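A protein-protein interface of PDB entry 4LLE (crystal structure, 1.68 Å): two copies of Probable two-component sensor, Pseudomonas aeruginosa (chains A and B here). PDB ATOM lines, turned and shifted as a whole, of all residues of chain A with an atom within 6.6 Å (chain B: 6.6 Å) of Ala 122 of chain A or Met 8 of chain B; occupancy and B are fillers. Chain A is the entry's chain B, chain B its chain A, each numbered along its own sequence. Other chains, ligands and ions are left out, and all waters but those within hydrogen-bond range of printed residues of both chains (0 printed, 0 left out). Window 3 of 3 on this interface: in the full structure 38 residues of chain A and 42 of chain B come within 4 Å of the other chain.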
ATOM      1  N   TYR A  12       0.756   8.228  -9.350  1.00  0.00           N
ATOM      2  CA  TYR A  12       1.015   7.607 -10.640  1.00  0.00           C
ATOM      3  C   TYR A  12       2.517   7.485 -10.882  1.00  0.00           C
ATOM      4  O   TYR A  12       2.966   6.577 -11.573  1.00  0.00           O
ATOM      5  CB  TYR A  12       0.331   8.382 -11.771  1.00  0.00           C
ATOM      6  CG  TYR A  12      -1.156   8.113 -11.886  1.00  0.00           C
ATOM      7  CD1 TYR A  12      -1.631   7.038 -12.624  1.00  0.00           C
ATOM      8  CD2 TYR A  12      -2.081   8.935 -11.257  1.00  0.00           C
ATOM      9  CE1 TYR A  12      -2.987   6.791 -12.731  1.00  0.00           C
ATOM     10  CE2 TYR A  12      -3.437   8.695 -11.358  1.00  0.00           C
ATOM     11  CZ  TYR A  12      -3.883   7.622 -12.097  1.00  0.00           C
ATOM     12  OH  TYR A  12      -5.234   7.377 -12.203  1.00  0.00           O
ATOM     13  N   ALA A 117      -4.860   3.548 -16.992  1.00  0.00           N
ATOM     14  CA  ALA A 117      -5.094   4.620 -17.946  1.00  0.00           C
ATOM     15  C   ALA A 117      -6.587   4.877 -17.998  1.00  0.00           C
ATOM     16  O   ALA A 117      -7.035   6.023 -18.099  1.00  0.00           O
ATOM     17  CB  ALA A 117      -4.559   4.235 -19.322  1.00  0.00           C
ATOM     18  N   GLY A 118      -7.360   3.799 -17.919  1.00  0.00           N
ATOM     19  CA  GLY A 118      -8.807   3.898 -17.914  1.00  0.00           C
ATOM     20  C   GLY A 118      -9.308   4.802 -16.805  1.00  0.00           C
ATOM     21  O   GLY A 118     -10.245   5.579 -16.999  1.00  0.00           O
ATOM     22  N   ILE A 119      -8.675   4.708 -15.638  1.00  0.00           N
ATOM     23  CA  ILE A 119      -9.063   5.527 -14.495  1.00  0.00           C
ATOM     24  C   ILE A 119      -8.662   6.988 -14.676  1.00  0.00           C
ATOM     25  O   ILE A 119      -9.404   7.889 -14.292  1.00  0.00           O
ATOM     26  CB  ILE A 119      -8.462   5.000 -13.180  1.00  0.00           C
ATOM     27  CG1 ILE A 119      -9.033   3.625 -12.847  1.00  0.00           C
ATOM     28  CG2 ILE A 119      -8.761   5.963 -12.034  1.00  0.00           C
ATOM     29  CD1 ILE A 119      -8.441   3.017 -11.605  1.00  0.00           C
ATOM     30  N   SER A 120      -7.488   7.225 -15.253  1.00  0.00           N
ATOM     31  CA  SER A 120      -7.036   8.593 -15.480  1.00  0.00           C
ATOM     32  C   SER A 120      -8.051   9.369 -16.305  1.00  0.00           C
ATOM     33  O   SER A 120      -8.426  10.483 -15.950  1.00  0.00           O
ATOM     34  CB  SER A 120      -5.664   8.618 -16.154  1.00  0.00           C
ATOM     35  OG  SER A 120      -4.654   8.233 -15.240  1.00  0.00           O
ATOM     36  N   GLU A 121      -8.498   8.772 -17.405  1.00  0.00           N
ATOM     37  CA  GLU A 121      -9.498   9.400 -18.260  1.00  0.00           C
ATOM     38  C   GLU A 121     -10.834   9.578 -17.541  1.00  0.00           C
ATOM     39  O   GLU A 121     -11.669  10.380 -17.959  1.00  0.00           O
ATOM     40  CB  GLU A 121      -9.682   8.609 -19.558  1.00  0.00           C
ATOM     41  CG  GLU A 121      -8.612   8.889 -20.605  1.00  0.00           C
ATOM     42  CD  GLU A 121      -7.778   7.667 -20.941  1.00  0.00           C
ATOM     43  OE1 GLU A 121      -6.570   7.830 -21.217  1.00  0.00           O
ATOM     44  OE2 GLU A 121      -8.329   6.547 -20.937  1.00  0.00           O
ATOM     45  N   ALA A 122     -11.029   8.833 -16.456  1.00  0.00           N
ATOM     46  CA  ALA A 122     -12.234   8.965 -15.644  1.00  0.00           C
ATOM     47  C   ALA A 122     -11.976   9.861 -14.433  1.00  0.00           C
ATOM     48  O   ALA A 122     -12.837  10.029 -13.570  1.00  0.00           O
ATOM     49  CB  ALA A 122     -12.734   7.598 -15.208  1.00  0.00           C
ATOM     50  N   GLU A 123     -10.771  10.418 -14.377  1.00  0.00           N
ATOM     51  CA  GLU A 123     -10.439  11.460 -13.416  1.00  0.00           C
ATOM     52  C   GLU A 123     -10.225  12.745 -14.198  1.00  0.00           C
ATOM     53  O   GLU A 123      -9.966  13.806 -13.630  1.00  0.00           O
ATOM     54  CB  GLU A 123      -9.194  11.086 -12.607  1.00  0.00           C
ATOM     55  CG  GLU A 123      -9.443   9.995 -11.573  1.00  0.00           C
ATOM     56  CD  GLU A 123      -8.179   9.564 -10.851  1.00  0.00           C
ATOM     57  OE1 GLU A 123      -8.295   8.949  -9.770  1.00  0.00           O
ATOM     58  OE2 GLU A 123      -7.071   9.837 -11.362  1.00  0.00           O
ATOM     59  N   THR A 124     -10.332  12.623 -15.518  1.00  0.00           N
ATOM     60  CA  THR A 124     -10.381  13.770 -16.412  1.00  0.00           C
ATOM     61  C   THR A 124     -11.805  14.303 -16.426  1.00  0.00           C
ATOM     62  O   THR A 124     -12.035  15.511 -16.376  1.00  0.00           O
ATOM     63  CB  THR A 124      -9.980  13.380 -17.846  1.00  0.00           C
ATOM     64  OG1 THR A 124      -8.552  13.295 -17.940  1.00  0.00           O
ATOM     65  CG2 THR A 124     -10.485  14.411 -18.844  1.00  0.00           C
ATOM     66  N   SER A 125     -12.762  13.384 -16.491  1.00  0.00           N
ATOM     67  CA  SER A 125     -14.174  13.737 -16.465  1.00  0.00           C
ATOM     68  C   SER A 125     -14.663  13.853 -15.026  1.00  0.00           C
ATOM     69  O   SER A 125     -15.682  13.270 -14.658  1.00  0.00           O
ATOM     70  CB  SER A 125     -14.999  12.691 -17.218  1.00  0.00           C
ATOM     71  OG  SER A 125     -15.794  13.295 -18.224  1.00  0.00           O
ATOM     72  N   ALA A 126     -13.930  14.611 -14.219  1.00  0.00           N
ATOM     73  CA  ALA A 126     -14.280  14.804 -12.817  1.00  0.00           C
ATOM     74  C   ALA A 126     -15.066  16.095 -12.613  1.00  0.00           C
ATOM     75  O   ALA A 126     -14.628  17.169 -13.024  1.00  0.00           O
ATOM     76  CB  ALA A 126     -13.024  14.802 -11.954  1.00  0.00           C
ATOM     77  N   GLN B   4     -18.966   7.914 -14.338  1.00  0.00           N
ATOM     78  CA  GLN B   4     -18.042   8.396 -13.318  1.00  0.00           C
ATOM     79  C   GLN B   4     -17.715   7.301 -12.305  1.00  0.00           C
ATOM     80  O   GLN B   4     -16.836   6.473 -12.540  1.00  0.00           O
ATOM     81  CB  GLN B   4     -18.616   9.620 -12.616  1.00  0.00           C
ATOM     82  N   GLU B   5     -18.432   7.300 -11.185  1.00  0.00           N
ATOM     83  CA  GLU B   5     -18.176   6.349 -10.104  1.00  0.00           C
ATOM     84  C   GLU B   5     -18.237   4.877 -10.533  1.00  0.00           C
ATOM     85  O   GLU B   5     -17.520   4.043  -9.980  1.00  0.00           O
ATOM     86  CB  GLU B   5     -19.116   6.603  -8.921  1.00  0.00           C
ATOM     87  CG  GLU B   5     -18.599   7.635  -7.924  1.00  0.00           C
ATOM     88  CD  GLU B   5     -18.325   8.984  -8.560  1.00  0.00           C
ATOM     89  OE1 GLU B   5     -19.162   9.447  -9.363  1.00  0.00           O
ATOM     90  OE2 GLU B   5     -17.270   9.582  -8.256  1.00  0.00           O
ATOM     91  N   GLN B   6     -19.091   4.555 -11.504  1.00  0.00           N
ATOM     92  CA  GLN B   6     -19.163   3.188 -12.018  1.00  0.00           C
ATOM     93  C   GLN B   6     -17.897   2.845 -12.788  1.00  0.00           C
ATOM     94  O   GLN B   6     -17.202   1.878 -12.469  1.00  0.00           O
ATOM     95  CB  GLN B   6     -20.364   3.005 -12.946  1.00  0.00           C
ATOM     96  CG  GLN B   6     -21.716   2.971 -12.265  1.00  0.00           C
ATOM     97  CD  GLN B   6     -22.813   2.519 -13.211  1.00  0.00           C
ATOM     98  OE1 GLN B   6     -22.549   1.816 -14.189  1.00  0.00           O
ATOM     99  NE2 GLN B   6     -24.046   2.924 -12.931  1.00  0.00           N
ATOM    100  N   ARG B   7     -17.615   3.645 -13.811  1.00  0.00           N
ATOM    101  CA  ARG B   7     -16.453   3.443 -14.665  1.00  0.00           C
ATOM    102  C   ARG B   7     -15.197   3.153 -13.847  1.00  0.00           C
ATOM    103  O   ARG B   7     -14.606   2.078 -13.974  1.00  0.00           O
ATOM    104  CB  ARG B   7     -16.237   4.664 -15.561  1.00  0.00           C
ATOM    105  CG  ARG B   7     -15.097   4.523 -16.560  1.00  0.00           C
ATOM    106  CD  ARG B   7     -15.612   4.527 -17.995  1.00  0.00           C
ATOM    107  NE  ARG B   7     -16.023   3.200 -18.448  1.00  0.00           N
ATOM    108  CZ  ARG B   7     -15.269   2.404 -19.202  1.00  0.00           C
ATOM    109  NH1 ARG B   7     -15.719   1.211 -19.571  1.00  0.00           N
ATOM    110  NH2 ARG B   7     -14.065   2.802 -19.589  1.00  0.00           N
ATOM    111  N   MET B   8     -14.800   4.103 -13.002  1.00  0.00           N
ATOM    112  CA  MET B   8     -13.581   3.955 -12.202  1.00  0.00           C
ATOM    113  C   MET B   8     -13.603   2.710 -11.321  1.00  0.00           C
ATOM    114  O   MET B   8     -12.574   2.059 -11.123  1.00  0.00           O
ATOM    115  CB  MET B   8     -13.338   5.195 -11.342  1.00  0.00           C
ATOM    116  CG  MET B   8     -12.779   6.381 -12.107  1.00  0.00           C
ATOM    117  SD  MET B   8     -12.447   7.918 -10.952  1.00  0.00           S
ATOM    118  CE  MET B   8     -11.261   7.065  -9.655  1.00  0.00           C
ATOM    119  N   SER B   9     -14.773   2.381 -10.783  1.00  0.00           N
ATOM    120  CA  SER B   9     -14.904   1.199  -9.940  1.00  0.00           C
ATOM    121  C   SER B   9     -14.594  -0.066 -10.739  1.00  0.00           C
ATOM    122  O   SER B   9     -13.987  -1.009 -10.223  1.00  0.00           O
ATOM    123  CB  SER B   9     -16.308   1.120  -9.335  1.00  0.00           C
ATOM    124  OG  SER B   9     -16.395   0.080  -8.375  1.00  0.00           O
ATOM    125  N   HIS B  10     -15.003  -0.072 -12.004  1.00  0.00           N
ATOM    126  CA  HIS B  10     -14.787  -1.220 -12.878  1.00  0.00           C
ATOM    127  C   HIS B  10     -13.303  -1.375 -13.193  1.00  0.00           C
ATOM    128  O   HIS B  10     -12.775  -2.483 -13.235  1.00  0.00           O
ATOM    129  CB  HIS B  10     -15.561  -1.055 -14.190  1.00  0.00           C
ATOM    130  CG  HIS B  10     -17.050  -1.086 -14.030  1.00  0.00           C
ATOM    131  ND1 HIS B  10     -17.671  -1.513 -12.875  1.00  0.00           N
ATOM    132  CD2 HIS B  10     -18.041  -0.744 -14.887  1.00  0.00           C
ATOM    133  CE1 HIS B  10     -18.982  -1.431 -13.027  1.00  0.00           C
ATOM    134  NE2 HIS B  10     -19.232  -0.969 -14.240  1.00  0.00           N
ATOM    135  N   HIS B  11     -12.630  -0.262 -13.434  1.00  0.00           N
ATOM    136  CA  HIS B  11     -11.227  -0.329 -13.804  1.00  0.00           C
ATOM    137  C   HIS B  11     -10.398  -0.769 -12.608  1.00  0.00           C
ATOM    138  O   HIS B  11      -9.426  -1.504 -12.761  1.00  0.00           O
ATOM    139  CB  HIS B  11     -10.742   1.011 -14.354  1.00  0.00           C
ATOM    140  CG  HIS B  11     -11.368   1.380 -15.664  1.00  0.00           C
ATOM    141  ND1 HIS B  11     -11.109   0.692 -16.830  1.00  0.00           N
ATOM    142  CD2 HIS B  11     -12.262   2.345 -15.987  1.00  0.00           C
ATOM    143  CE1 HIS B  11     -11.799   1.230 -17.819  1.00  0.00           C
ATOM    144  NE2 HIS B  11     -12.510   2.232 -17.334  1.00  0.00           N
ATOM    145  N   TYR B  12     -10.784  -0.314 -11.420  1.00  0.00           N
ATOM    146  CA  TYR B  12     -10.105  -0.751 -10.203  1.00  0.00           C
ATOM    147  C   TYR B  12     -10.228  -2.256 -10.009  1.00  0.00           C
ATOM    148  O   TYR B  12      -9.261  -2.919  -9.624  1.00  0.00           O
ATOM    149  CB  TYR B  12     -10.644  -0.034  -8.968  1.00  0.00           C
ATOM    150  CG  TYR B  12      -9.965   1.277  -8.670  1.00  0.00           C
ATOM    151  CD1 TYR B  12      -8.650   1.316  -8.232  1.00  0.00           C
ATOM    152  CD2 TYR B  12     -10.648   2.478  -8.806  1.00  0.00           C
ATOM    153  CE1 TYR B  12      -8.026   2.525  -7.954  1.00  0.00           C
ATOM    154  CE2 TYR B  12     -10.038   3.685  -8.530  1.00  0.00           C
ATOM    155  CZ  TYR B  12      -8.730   3.705  -8.106  1.00  0.00           C
ATOM    156  OH  TYR B  12      -8.130   4.911  -7.831  1.00  0.00           O
ATOM    157  N   ALA B  13     -11.414  -2.797 -10.264  1.00  0.00           N
ATOM    158  CA  ALA B  13     -11.624  -4.237 -10.114  1.00  0.00           C
ATOM    159  C   ALA B  13     -10.669  -5.002 -11.018  1.00  0.00           C
ATOM    160  O   ALA B  13     -10.106  -6.023 -10.623  1.00  0.00           O
ATOM    161  CB  ALA B  13     -13.066  -4.618 -10.413  1.00  0.00           C
ATOM    162  N   ILE B 119      -4.624   6.532  -4.640  1.00  0.00           N
ATOM    163  CA  ILE B 119      -5.388   7.125  -5.731  1.00  0.00           C
ATOM    164  C   ILE B 119      -6.878   6.970  -5.479  1.00  0.00           C
ATOM    165  O   ILE B 119      -7.653   7.908  -5.665  1.00  0.00           O
ATOM    166  CB  ILE B 119      -5.067   6.463  -7.085  1.00  0.00           C
ATOM    167  CG1 ILE B 119      -3.594   6.637  -7.443  1.00  0.00           C
ATOM    168  CG2 ILE B 119      -5.941   7.047  -8.185  1.00  0.00           C
ATOM    169  CD1 ILE B 119      -3.276   6.209  -8.855  1.00  0.00           C
ATOM    170  N   SER B 120      -7.272   5.774  -5.055  1.00  0.00           N
ATOM    171  CA  SER B 120      -8.675   5.470  -4.802  1.00  0.00           C
ATOM    172  C   SER B 120      -9.246   6.284  -3.642  1.00  0.00           C
ATOM    173  O   SER B 120     -10.238   6.997  -3.804  1.00  0.00           O
ATOM    174  CB  SER B 120      -8.857   3.971  -4.540  1.00  0.00           C
ATOM    175  OG  SER B 120     -10.210   3.658  -4.252  1.00  0.00           O
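Of the 11 printed residues of chain A, 5 touch a printed residue of chain B.
Among the printed residues, 8 pairs touch across the chains.
Among the printed residues, no Asp or Glu carboxylate lies within 4 Å of a Lys or Arg side-chain nitrogen of the other chain.
Of the printed residues of chain B, Glu 123 of chain A touches Met 8 and Ile 119.
Of the printed residues of chain A, His 11 of chain B touches Gly 118 (3.9 Å) and Ile 119 (3.5 Å).
Printed residues of chain B within 4 Å of Gly 118 of chain A: His 11 (3.9 Å).
Ala 126 of chain A touches none of the printed residues of chain B.
The nearest printed residue of chain B that does not touch Ile 119 of chain A is Ile 119 of chain B (4.9 Å).
The side-chain sulfur (SD) of Met 8 of chain B sits close to the backbone carbonyl oxygen (O) of Ala 122 of chain A, 3.4 Å away.
Among the printed residues, merely in contact across the chains: Glu 123 of chain A with Ile 119 of chain B, Ile 119 of chain A with His 11 of chain B, Glu 123 of chain A with Met 8 of chain B, Ile 119 of chain A with Tyr 12 of chain B, Tyr 12 of chain A with Ile 119 of chain B, Ile 119 of chain A with Met 8 of chain B and Gly 118 of chain A with His 11 of chain B.
OG of Ser 120 of chain A is in hydrogen-bond range of OH of Tyr 12 of chain A (3.2 Å).
The side-chain hydroxyl (OH) of Tyr 12 of chain A sits at hydrogen-bond distance from the side-chain carboxylate (OE2) of Glu 123 of chain A, at 3.2 Å.
The guanidinium group (NH2) of Arg 7 of chain B sits at hydrogen-bond distance from a ring nitrogen (NE2) of His 11 of chain B, 2.8 Å away.
The side-chain hydroxyl (OH) of Tyr 12 of chain B lies within hydrogen-bond range of the backbone NH (N) of Ser 120 of chain B (3.0 Å).
Tyr 12 of chain A touches Ile 119 of chain B, and with the chains exchanged Ile 119 of chain A touches Tyr 12 of chain B.
3 positions are printed for both chains.
Of the 8 pairs that touch across the chains among the printed residues, 2 have their exchanged pair printed and touching as well.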
